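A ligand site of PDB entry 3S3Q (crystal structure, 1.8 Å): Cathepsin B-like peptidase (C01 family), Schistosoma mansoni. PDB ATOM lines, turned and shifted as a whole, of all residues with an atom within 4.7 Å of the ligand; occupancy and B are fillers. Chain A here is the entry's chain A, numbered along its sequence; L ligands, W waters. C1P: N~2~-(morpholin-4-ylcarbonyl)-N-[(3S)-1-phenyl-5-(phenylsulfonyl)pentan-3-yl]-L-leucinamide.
The backbone carbonyl oxygen of Gly 75 lies within hydrogen-bond range of a nitrogen (N1) of the ligand, at 3.0 Å.
The indole nitrogen (NE1) of Trp 223 lies within hydrogen-bond range of an oxygen (O34) of the ligand, at 3.4 Å.
C18 of the ligand is bonded to SG of Cys 31 (2.0 Å).
The backbone NH of Gly 75 is in hydrogen-bond range of an oxygen (O4) of the ligand (2.9 Å).
O of Gly 200 sits at hydrogen-bond distance from N28 of the ligand (3.1 Å).
The side-chain amide nitrogen (NE2) of Gln 25 lies within hydrogen-bond range of an oxygen (O34) of the ligand, at 3.0 Å.
O of Gly 29 touches C19 of the ligand (3.3 Å).
CD1 of Trp 32 touches O4 of the ligand, 3.4 Å away.
Leu 70 touches the ligand (CD1 to C11, 3.8 Å).
O of Cys 72 touches C23 of the ligand, 3.6 Å away.
O of Glu 73 touches C11 of the ligand, at 3.3 Å.
CA of Gly 74 touches O4 of the ligand, at 3.1 Å.
Leu 77 touches the ligand.
CD1 of Ile 124 touches C24 of the ligand, at 3.2 Å.
Val 178 touches the ligand (CG2 to C37, 3.2 Å).
CD2 of Leu 183 touches C29 of the ligand, at 3.8 Å.
His 201 touches the ligand.
Glu 247 touches the ligand.
Water W1 bridges O16 of the ligand (2.7 Å) and N of Gly 200 (2.9 Å).
The side-chain amide nitrogen (NE2) of Gln 25 sits close to the indole nitrogen (NE1) of Trp 223 (3.3 Å).
The side-chain sulfur (SG) of Cys 31 lies within hydrogen-bond range of the backbone NH (N) of Ala 202 (3.6 Å).
The side-chain sulfur (SG) of Cys 31 lies close to a ring nitrogen (ND1) of His 201, at 3.6 Å.
OE1 of Gln 25 is in hydrogen-bond range of N of Cys 31, at 2.7 Å.
The backbone carbonyl oxygen of Cys 72 sits at hydrogen-bond distance from the backbone NH of Gly 29, 2.8 Å away.
N of Gly 175 lies within hydrogen-bond range of O of Glu 247 (3.0 Å).
O of Val 178 lies within hydrogen-bond range of N of Leu 198.
The side-chain amide oxygen (OE1) of Gln 25 is in hydrogen-bond range of the backbone NH (N) of Ser 30 (3.1 Å).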
ATOM      1  N   GLN A  25       4.566   6.068 -17.795  1.00  0.00           N
ATOM      2  CA  GLN A  25       4.516   7.395 -17.170  1.00  0.00           C
ATOM      3  C   GLN A  25       5.096   8.501 -18.041  1.00  0.00           C
ATOM      4  O   GLN A  25       4.809   9.679 -17.808  1.00  0.00           O
ATOM      5  CB  GLN A  25       5.353   7.421 -15.887  1.00  0.00           C
ATOM      6  CG  GLN A  25       4.899   6.492 -14.764  1.00  0.00           C
ATOM      7  CD  GLN A  25       5.978   6.435 -13.713  1.00  0.00           C
ATOM      8  OE1 GLN A  25       6.335   7.461 -13.122  1.00  0.00           O
ATOM      9  NE2 GLN A  25       6.526   5.256 -13.500  1.00  0.00           N
ATOM     10  N   GLY A  29       7.166  11.946 -12.960  1.00  0.00           N
ATOM     11  CA  GLY A  29       7.176  11.070 -11.772  1.00  0.00           C
ATOM     12  C   GLY A  29       5.778  10.712 -11.316  1.00  0.00           C
ATOM     13  O   GLY A  29       5.431  10.925 -10.163  1.00  0.00           O
ATOM     14  N   SER A  30       4.985  10.156 -12.224  1.00  0.00           N
ATOM     15  CA  SER A  30       3.560   9.914 -11.970  1.00  0.00           C
ATOM     16  C   SER A  30       3.270   8.468 -11.587  1.00  0.00           C
ATOM     17  O   SER A  30       2.099   8.038 -11.586  1.00  0.00           O
ATOM     18  CB  SER A  30       2.745  10.291 -13.207  1.00  0.00           C
ATOM     19  OG  SER A  30       3.242   9.628 -14.371  1.00  0.00           O
ATOM     20  N   CYS A  31       4.325   7.709 -11.266  1.00  0.00           N
ATOM     21  CA  CYS A  31       4.167   6.329 -10.825  1.00  0.00           C
ATOM     22  C   CYS A  31       3.071   6.149  -9.792  1.00  0.00           C
ATOM     23  O   CYS A  31       2.295   5.200  -9.863  1.00  0.00           O
ATOM     24  CB  CYS A  31       5.474   5.798 -10.237  1.00  0.00           C
ATOM     25  SG  CYS A  31       6.067   6.702  -8.785  1.00  0.00           S
ATOM     26  N   TRP A  32       3.001   7.074  -8.836  1.00  0.00           N
ATOM     27  CA  TRP A  32       1.999   7.014  -7.769  1.00  0.00           C
ATOM     28  C   TRP A  32       0.580   6.968  -8.347  1.00  0.00           C
ATOM     29  O   TRP A  32      -0.304   6.259  -7.811  1.00  0.00           O
ATOM     30  CB  TRP A  32       2.163   8.231  -6.829  1.00  0.00           C
ATOM     31  CG  TRP A  32       1.839   9.572  -7.500  1.00  0.00           C
ATOM     32  CD1 TRP A  32       2.706  10.431  -8.141  1.00  0.00           C
ATOM     33  CD2 TRP A  32       0.559  10.182  -7.569  1.00  0.00           C
ATOM     34  NE1 TRP A  32       2.024  11.543  -8.579  1.00  0.00           N
ATOM     35  CE2 TRP A  32       0.708  11.406  -8.250  1.00  0.00           C
ATOM     36  CE3 TRP A  32      -0.715   9.818  -7.086  1.00  0.00           C
ATOM     37  CZ2 TRP A  32      -0.370  12.258  -8.490  1.00  0.00           C
ATOM     38  CZ3 TRP A  32      -1.787  10.659  -7.338  1.00  0.00           C
ATOM     39  CH2 TRP A  32      -1.612  11.868  -8.041  1.00  0.00           C
ATOM     40  N   LEU A  70       2.888  16.203  -5.337  1.00  0.00           N
ATOM     41  CA  LEU A  70       3.504  17.164  -6.247  1.00  0.00           C
ATOM     42  C   LEU A  70       3.397  16.795  -7.726  1.00  0.00           C
ATOM     43  O   LEU A  70       4.201  17.261  -8.546  1.00  0.00           O
ATOM     44  CB  LEU A  70       4.974  17.361  -5.866  1.00  0.00           C
ATOM     45  CG  LEU A  70       5.307  17.676  -4.401  1.00  0.00           C
ATOM     46  CD1 LEU A  70       6.816  17.933  -4.260  1.00  0.00           C
ATOM     47  CD2 LEU A  70       4.480  18.855  -3.847  1.00  0.00           C
ATOM     48  N   CYS A  72       3.819  15.529 -11.222  1.00  0.00           N
ATOM     49  CA  CYS A  72       4.953  14.904 -11.885  1.00  0.00           C
ATOM     50  C   CYS A  72       6.193  14.845 -10.992  1.00  0.00           C
ATOM     51  O   CYS A  72       7.139  14.160 -11.321  1.00  0.00           O
ATOM     52  CB  CYS A  72       5.295  15.597 -13.204  1.00  0.00           C
ATOM     53  SG  CYS A  72       4.174  15.159 -14.548  1.00  0.00           S
ATOM     54  N   GLU A  73       6.216  15.570  -9.880  1.00  0.00           N
ATOM     55  CA  GLU A  73       7.349  15.483  -8.961  1.00  0.00           C
ATOM     56  C   GLU A  73       7.129  14.472  -7.838  1.00  0.00           C
ATOM     57  O   GLU A  73       7.911  14.386  -6.890  1.00  0.00           O
ATOM     58  CB  GLU A  73       7.737  16.858  -8.406  1.00  0.00           C
ATOM     59  CG  GLU A  73       8.618  17.684  -9.358  1.00  0.00           C
ATOM     60  CD  GLU A  73       8.840  19.112  -8.874  1.00  0.00           C
ATOM     61  OE1 GLU A  73       7.860  19.767  -8.456  1.00  0.00           O
ATOM     62  OE2 GLU A  73      10.003  19.572  -8.919  1.00  0.00           O
ATOM     63  N   GLY A  74       6.044  13.695  -7.944  1.00  0.00           N
ATOM     64  CA  GLY A  74       5.826  12.592  -7.028  1.00  0.00           C
ATOM     65  C   GLY A  74       4.635  12.789  -6.142  1.00  0.00           C
ATOM     66  O   GLY A  74       4.204  13.922  -5.914  1.00  0.00           O
ATOM     67  N   GLY A  75       4.120  11.676  -5.639  1.00  0.00           N
ATOM     68  CA  GLY A  75       2.842  11.664  -4.943  1.00  0.00           C
ATOM     69  C   GLY A  75       2.706  10.702  -3.774  1.00  0.00           C
ATOM     70  O   GLY A  75       3.698  10.089  -3.310  1.00  0.00           O
ATOM     71  N   ILE A  76       1.468  10.577  -3.312  1.00  0.00           N
ATOM     72  CA  ILE A  76       1.138   9.937  -2.038  1.00  0.00           C
ATOM     73  C   ILE A  76      -0.050   8.990  -2.250  1.00  0.00           C
ATOM     74  O   ILE A  76      -1.083   9.408  -2.776  1.00  0.00           O
ATOM     75  CB  ILE A  76       0.710  11.000  -0.972  1.00  0.00           C
ATOM     76  CG1 ILE A  76       1.662  12.219  -1.002  1.00  0.00           C
ATOM     77  CG2 ILE A  76       0.573  10.355   0.447  1.00  0.00           C
ATOM     78  CD1 ILE A  76       1.142  13.432  -0.227  1.00  0.00           C
ATOM     79  N   LEU A  77       0.088   7.735  -1.827  1.00  0.00           N
ATOM     80  CA  LEU A  77      -0.860   6.691  -2.231  1.00  0.00           C
ATOM     81  C   LEU A  77      -2.223   6.802  -1.558  1.00  0.00           C
ATOM     82  O   LEU A  77      -3.252   6.648  -2.202  1.00  0.00           O
ATOM     83  CB  LEU A  77      -0.254   5.295  -1.981  1.00  0.00           C
ATOM     84  CG  LEU A  77       1.043   4.945  -2.697  1.00  0.00           C
ATOM     85  CD1 LEU A  77       1.328   3.430  -2.529  1.00  0.00           C
ATOM     86  CD2 LEU A  77       1.065   5.394  -4.167  1.00  0.00           C
ATOM     87  N   ILE A 124      11.903  16.336 -16.533  1.00  0.00           N
ATOM     88  CA  ILE A 124      10.517  15.978 -16.184  1.00  0.00           C
ATOM     89  C   ILE A 124       9.564  17.081 -16.660  1.00  0.00           C
ATOM     90  O   ILE A 124       9.880  18.278 -16.510  1.00  0.00           O
ATOM     91  CB  ILE A 124      10.420  15.827 -14.639  1.00  0.00           C
ATOM     92  CG1 ILE A 124      11.522  14.874 -14.135  1.00  0.00           C
ATOM     93  CG2 ILE A 124       9.008  15.435 -14.193  1.00  0.00           C
ATOM     94  CD1 ILE A 124      11.122  13.978 -13.003  1.00  0.00           C
ATOM     95  N   GLY A 175       4.106   0.769  -2.662  1.00  0.00           N
ATOM     96  CA  GLY A 175       5.268   1.648  -2.725  1.00  0.00           C
ATOM     97  C   GLY A 175       6.496   0.839  -2.340  1.00  0.00           C
ATOM     98  O   GLY A 175       6.406  -0.124  -1.557  1.00  0.00           O
ATOM     99  N   VAL A 178      13.442   2.557  -4.198  1.00  0.00           N
ATOM    100  CA  VAL A 178      14.170   2.350  -5.419  1.00  0.00           C
ATOM    101  C   VAL A 178      15.620   2.794  -5.251  1.00  0.00           C
ATOM    102  O   VAL A 178      15.900   3.923  -4.815  1.00  0.00           O
ATOM    103  CB  VAL A 178      13.465   3.004  -6.643  1.00  0.00           C
ATOM    104  CG1 VAL A 178      13.355   4.536  -6.513  1.00  0.00           C
ATOM    105  CG2 VAL A 178      14.148   2.581  -7.952  1.00  0.00           C
ATOM    106  N   PHE A 182      18.157  -0.708  -9.412  1.00  0.00           N
ATOM    107  CA  PHE A 182      16.864  -0.929 -10.060  1.00  0.00           C
ATOM    108  C   PHE A 182      16.866  -0.443 -11.526  1.00  0.00           C
ATOM    109  O   PHE A 182      16.288  -1.107 -12.404  1.00  0.00           O
ATOM    110  CB  PHE A 182      15.714  -0.297  -9.262  1.00  0.00           C
ATOM    111  CG  PHE A 182      14.344  -0.617  -9.815  1.00  0.00           C
ATOM    112  CD1 PHE A 182      13.684  -1.797  -9.472  1.00  0.00           C
ATOM    113  CD2 PHE A 182      13.725   0.266 -10.693  1.00  0.00           C
ATOM    114  CE1 PHE A 182      12.425  -2.086  -9.971  1.00  0.00           C
ATOM    115  CE2 PHE A 182      12.452  -0.011 -11.203  1.00  0.00           C
ATOM    116  CZ  PHE A 182      11.810  -1.180 -10.854  1.00  0.00           C
ATOM    117  N   LEU A 183      17.535   0.684 -11.783  1.00  0.00           N
ATOM    118  CA  LEU A 183      17.655   1.228 -13.148  1.00  0.00           C
ATOM    119  C   LEU A 183      18.315   0.281 -14.138  1.00  0.00           C
ATOM    120  O   LEU A 183      18.170   0.439 -15.385  1.00  0.00           O
ATOM    121  CB  LEU A 183      18.439   2.539 -13.149  1.00  0.00           C
ATOM    122  CG  LEU A 183      17.797   3.682 -12.378  1.00  0.00           C
ATOM    123  CD1 LEU A 183      18.425   5.008 -12.812  1.00  0.00           C
ATOM    124  CD2 LEU A 183      16.264   3.712 -12.543  1.00  0.00           C
ATOM    125  N   LEU A 198      17.203   6.320  -4.708  1.00  0.00           N
ATOM    126  CA  LEU A 198      16.658   7.277  -5.634  1.00  0.00           C
ATOM    127  C   LEU A 198      15.273   7.685  -5.205  1.00  0.00           C
ATOM    128  O   LEU A 198      14.525   8.261  -5.990  1.00  0.00           O
ATOM    129  CB  LEU A 198      16.637   6.712  -7.054  1.00  0.00           C
ATOM    130  CG  LEU A 198      18.007   6.385  -7.669  1.00  0.00           C
ATOM    131  CD1 LEU A 198      17.807   5.595  -8.948  1.00  0.00           C
ATOM    132  CD2 LEU A 198      18.791   7.655  -7.938  1.00  0.00           C
ATOM    133  N   GLY A 200      11.418   6.828  -3.822  1.00  0.00           N
ATOM    134  CA  GLY A 200      10.399   5.773  -3.871  1.00  0.00           C
ATOM    135  C   GLY A 200       9.714   5.627  -5.210  1.00  0.00           C
ATOM    136  O   GLY A 200       9.726   6.530  -6.051  1.00  0.00           O
ATOM    137  N   HIS A 201       9.116   4.458  -5.415  1.00  0.00           N
ATOM    138  CA  HIS A 201       8.434   4.141  -6.654  1.00  0.00           C
ATOM    139  C   HIS A 201       7.161   3.438  -6.249  1.00  0.00           C
ATOM    140  O   HIS A 201       7.101   2.835  -5.169  1.00  0.00           O
ATOM    141  CB  HIS A 201       9.347   3.244  -7.507  1.00  0.00           C
ATOM    142  CG  HIS A 201       8.817   2.897  -8.863  1.00  0.00           C
ATOM    143  ND1 HIS A 201       7.798   3.581  -9.483  1.00  0.00           N
ATOM    144  CD2 HIS A 201       9.203   1.925  -9.734  1.00  0.00           C
ATOM    145  CE1 HIS A 201       7.565   3.046 -10.671  1.00  0.00           C
ATOM    146  NE2 HIS A 201       8.406   2.049 -10.852  1.00  0.00           N
ATOM    147  N   ALA A 202       6.121   3.570  -7.069  1.00  0.00           N
ATOM    148  CA  ALA A 202       4.811   2.993  -6.767  1.00  0.00           C
ATOM    149  C   ALA A 202       4.432   2.170  -7.978  1.00  0.00           C
ATOM    150  O   ALA A 202       4.517   2.645  -9.101  1.00  0.00           O
ATOM    151  CB  ALA A 202       3.770   4.095  -6.528  1.00  0.00           C
ATOM    152  N   TRP A 223       6.671   1.623 -17.148  1.00  0.00           N
ATOM    153  CA  TRP A 223       7.741   2.152 -17.978  1.00  0.00           C
ATOM    154  C   TRP A 223       7.742   1.545 -19.386  1.00  0.00           C
ATOM    155  O   TRP A 223       8.801   1.395 -20.009  1.00  0.00           O
ATOM    156  CB  TRP A 223       9.057   1.898 -17.260  1.00  0.00           C
ATOM    157  CG  TRP A 223       9.404   2.975 -16.258  1.00  0.00           C
ATOM    158  CD1 TRP A 223       8.695   4.120 -15.978  1.00  0.00           C
ATOM    159  CD2 TRP A 223      10.576   3.028 -15.463  1.00  0.00           C
ATOM    160  NE1 TRP A 223       9.369   4.869 -15.031  1.00  0.00           N
ATOM    161  CE2 TRP A 223      10.536   4.229 -14.717  1.00  0.00           C
ATOM    162  CE3 TRP A 223      11.683   2.174 -15.328  1.00  0.00           C
ATOM    163  CZ2 TRP A 223      11.554   4.589 -13.824  1.00  0.00           C
ATOM    164  CZ3 TRP A 223      12.686   2.533 -14.450  1.00  0.00           C
ATOM    165  CH2 TRP A 223      12.614   3.731 -13.694  1.00  0.00           C
ATOM    166  N   GLU A 247       4.069  -0.900   2.173  1.00  0.00           N
ATOM    167  CA  GLU A 247       3.319   0.264   1.679  1.00  0.00           C
ATOM    168  C   GLU A 247       2.274  -0.141   0.637  1.00  0.00           C
ATOM    169  O   GLU A 247       2.107   0.490  -0.438  1.00  0.00           O
ATOM    170  CB  GLU A 247       4.251   1.374   1.172  1.00  0.00           C
ATOM    171  CG  GLU A 247       3.582   2.744   1.085  1.00  0.00           C
ATOM    172  CD  GLU A 247       4.516   3.835   0.590  1.00  0.00           C
ATOM    173  OE1 GLU A 247       5.660   3.519   0.216  1.00  0.00           O
ATOM    174  OE2 GLU A 247       4.116   5.012   0.581  1.00  0.00           O
HETATM  175  N1  C1P L   1       6.549   9.756  -4.078  1.00  0.00           N
HETATM  176  C15 C1P L   1       7.442  10.753  -4.153  1.00  0.00           C
HETATM  177  O16 C1P L   1       8.415  10.630  -4.889  1.00  0.00           O
HETATM  178  N9  C1P L   1       7.285  11.889  -3.448  1.00  0.00           N
HETATM  179  C14 C1P L   1       6.150  12.070  -2.521  1.00  0.00           C
HETATM  180  C13 C1P L   1       5.598  13.496  -2.689  1.00  0.00           C
HETATM  181  O12 C1P L   1       6.690  14.397  -2.490  1.00  0.00           O
HETATM  182  C11 C1P L   1       7.624  14.321  -3.569  1.00  0.00           C
HETATM  183  C10 C1P L   1       8.302  12.956  -3.562  1.00  0.00           C
HETATM  184  C2  C1P L   1       6.706   8.524  -4.873  1.00  0.00           C
HETATM  185  C3  C1P L   1       6.640   8.900  -6.342  1.00  0.00           C
HETATM  186  O4  C1P L   1       5.648   9.509  -6.732  1.00  0.00           O
HETATM  187  N28 C1P L   1       7.668   8.585  -7.155  1.00  0.00           N
HETATM  188  C19 C1P L   1       7.637   8.968  -8.584  1.00  0.00           C
HETATM  189  C18 C1P L   1       7.640   7.696  -9.466  1.00  0.00           C
HETATM  190  C17 C1P L   1       8.890   6.810  -9.398  1.00  0.00           C
HETATM  191  S33 C1P L   1       9.652   6.687 -10.886  1.00  0.00           S
HETATM  192  O34 C1P L   1       8.891   5.936 -11.838  1.00  0.00           O
HETATM  193  O35 C1P L   1       9.885   8.000 -11.419  1.00  0.00           O
HETATM  194  C32 C1P L   1      11.101   6.082 -10.589  1.00  0.00           C
HETATM  195  C36 C1P L   1      11.343   4.706 -10.513  1.00  0.00           C
HETATM  196  C37 C1P L   1      12.648   4.255 -10.261  1.00  0.00           C
HETATM  197  C29 C1P L   1      13.693   5.156 -10.097  1.00  0.00           C
HETATM  198  C30 C1P L   1      13.456   6.538 -10.167  1.00  0.00           C
HETATM  199  C31 C1P L   1      12.156   6.993 -10.412  1.00  0.00           C
HETATM  200  C20 C1P L   1       8.872   9.803  -8.867  1.00  0.00           C
HETATM  201  C21 C1P L   1       8.732  11.218  -8.295  1.00  0.00           C
HETATM  202  C22 C1P L   1       9.970  12.047  -8.519  1.00  0.00           C
HETATM  203  C23 C1P L   1      10.014  12.935  -9.600  1.00  0.00           C
HETATM  204  C24 C1P L   1      11.141  13.741  -9.813  1.00  0.00           C
HETATM  205  C25 C1P L   1      12.217  13.630  -8.948  1.00  0.00           C
HETATM  206  C26 C1P L   1      12.178  12.746  -7.861  1.00  0.00           C
HETATM  207  C27 C1P L   1      11.055  11.945  -7.640  1.00  0.00           C
HETATM  208  C5  C1P L   1       5.540   7.594  -4.561  1.00  0.00           C
HETATM  209  C6  C1P L   1       5.654   6.939  -3.175  1.00  0.00           C
HETATM  210  C7  C1P L   1       6.909   6.097  -3.042  1.00  0.00           C
HETATM  211  C8  C1P L   1       4.479   6.026  -2.911  1.00  0.00           C
HETATM  212  O   HOH W   1      10.839   9.674  -4.211  1.00  0.00           O
HETATM  213  O   HOH W   2       6.837  15.870  -0.270  1.00  0.00           O
HETATM  214  O   HOH W   3      11.989  10.611 -11.389  1.00  0.00           O
HETATM  215  O   HOH W   4      12.967   9.778  -8.997  1.00  0.00           O
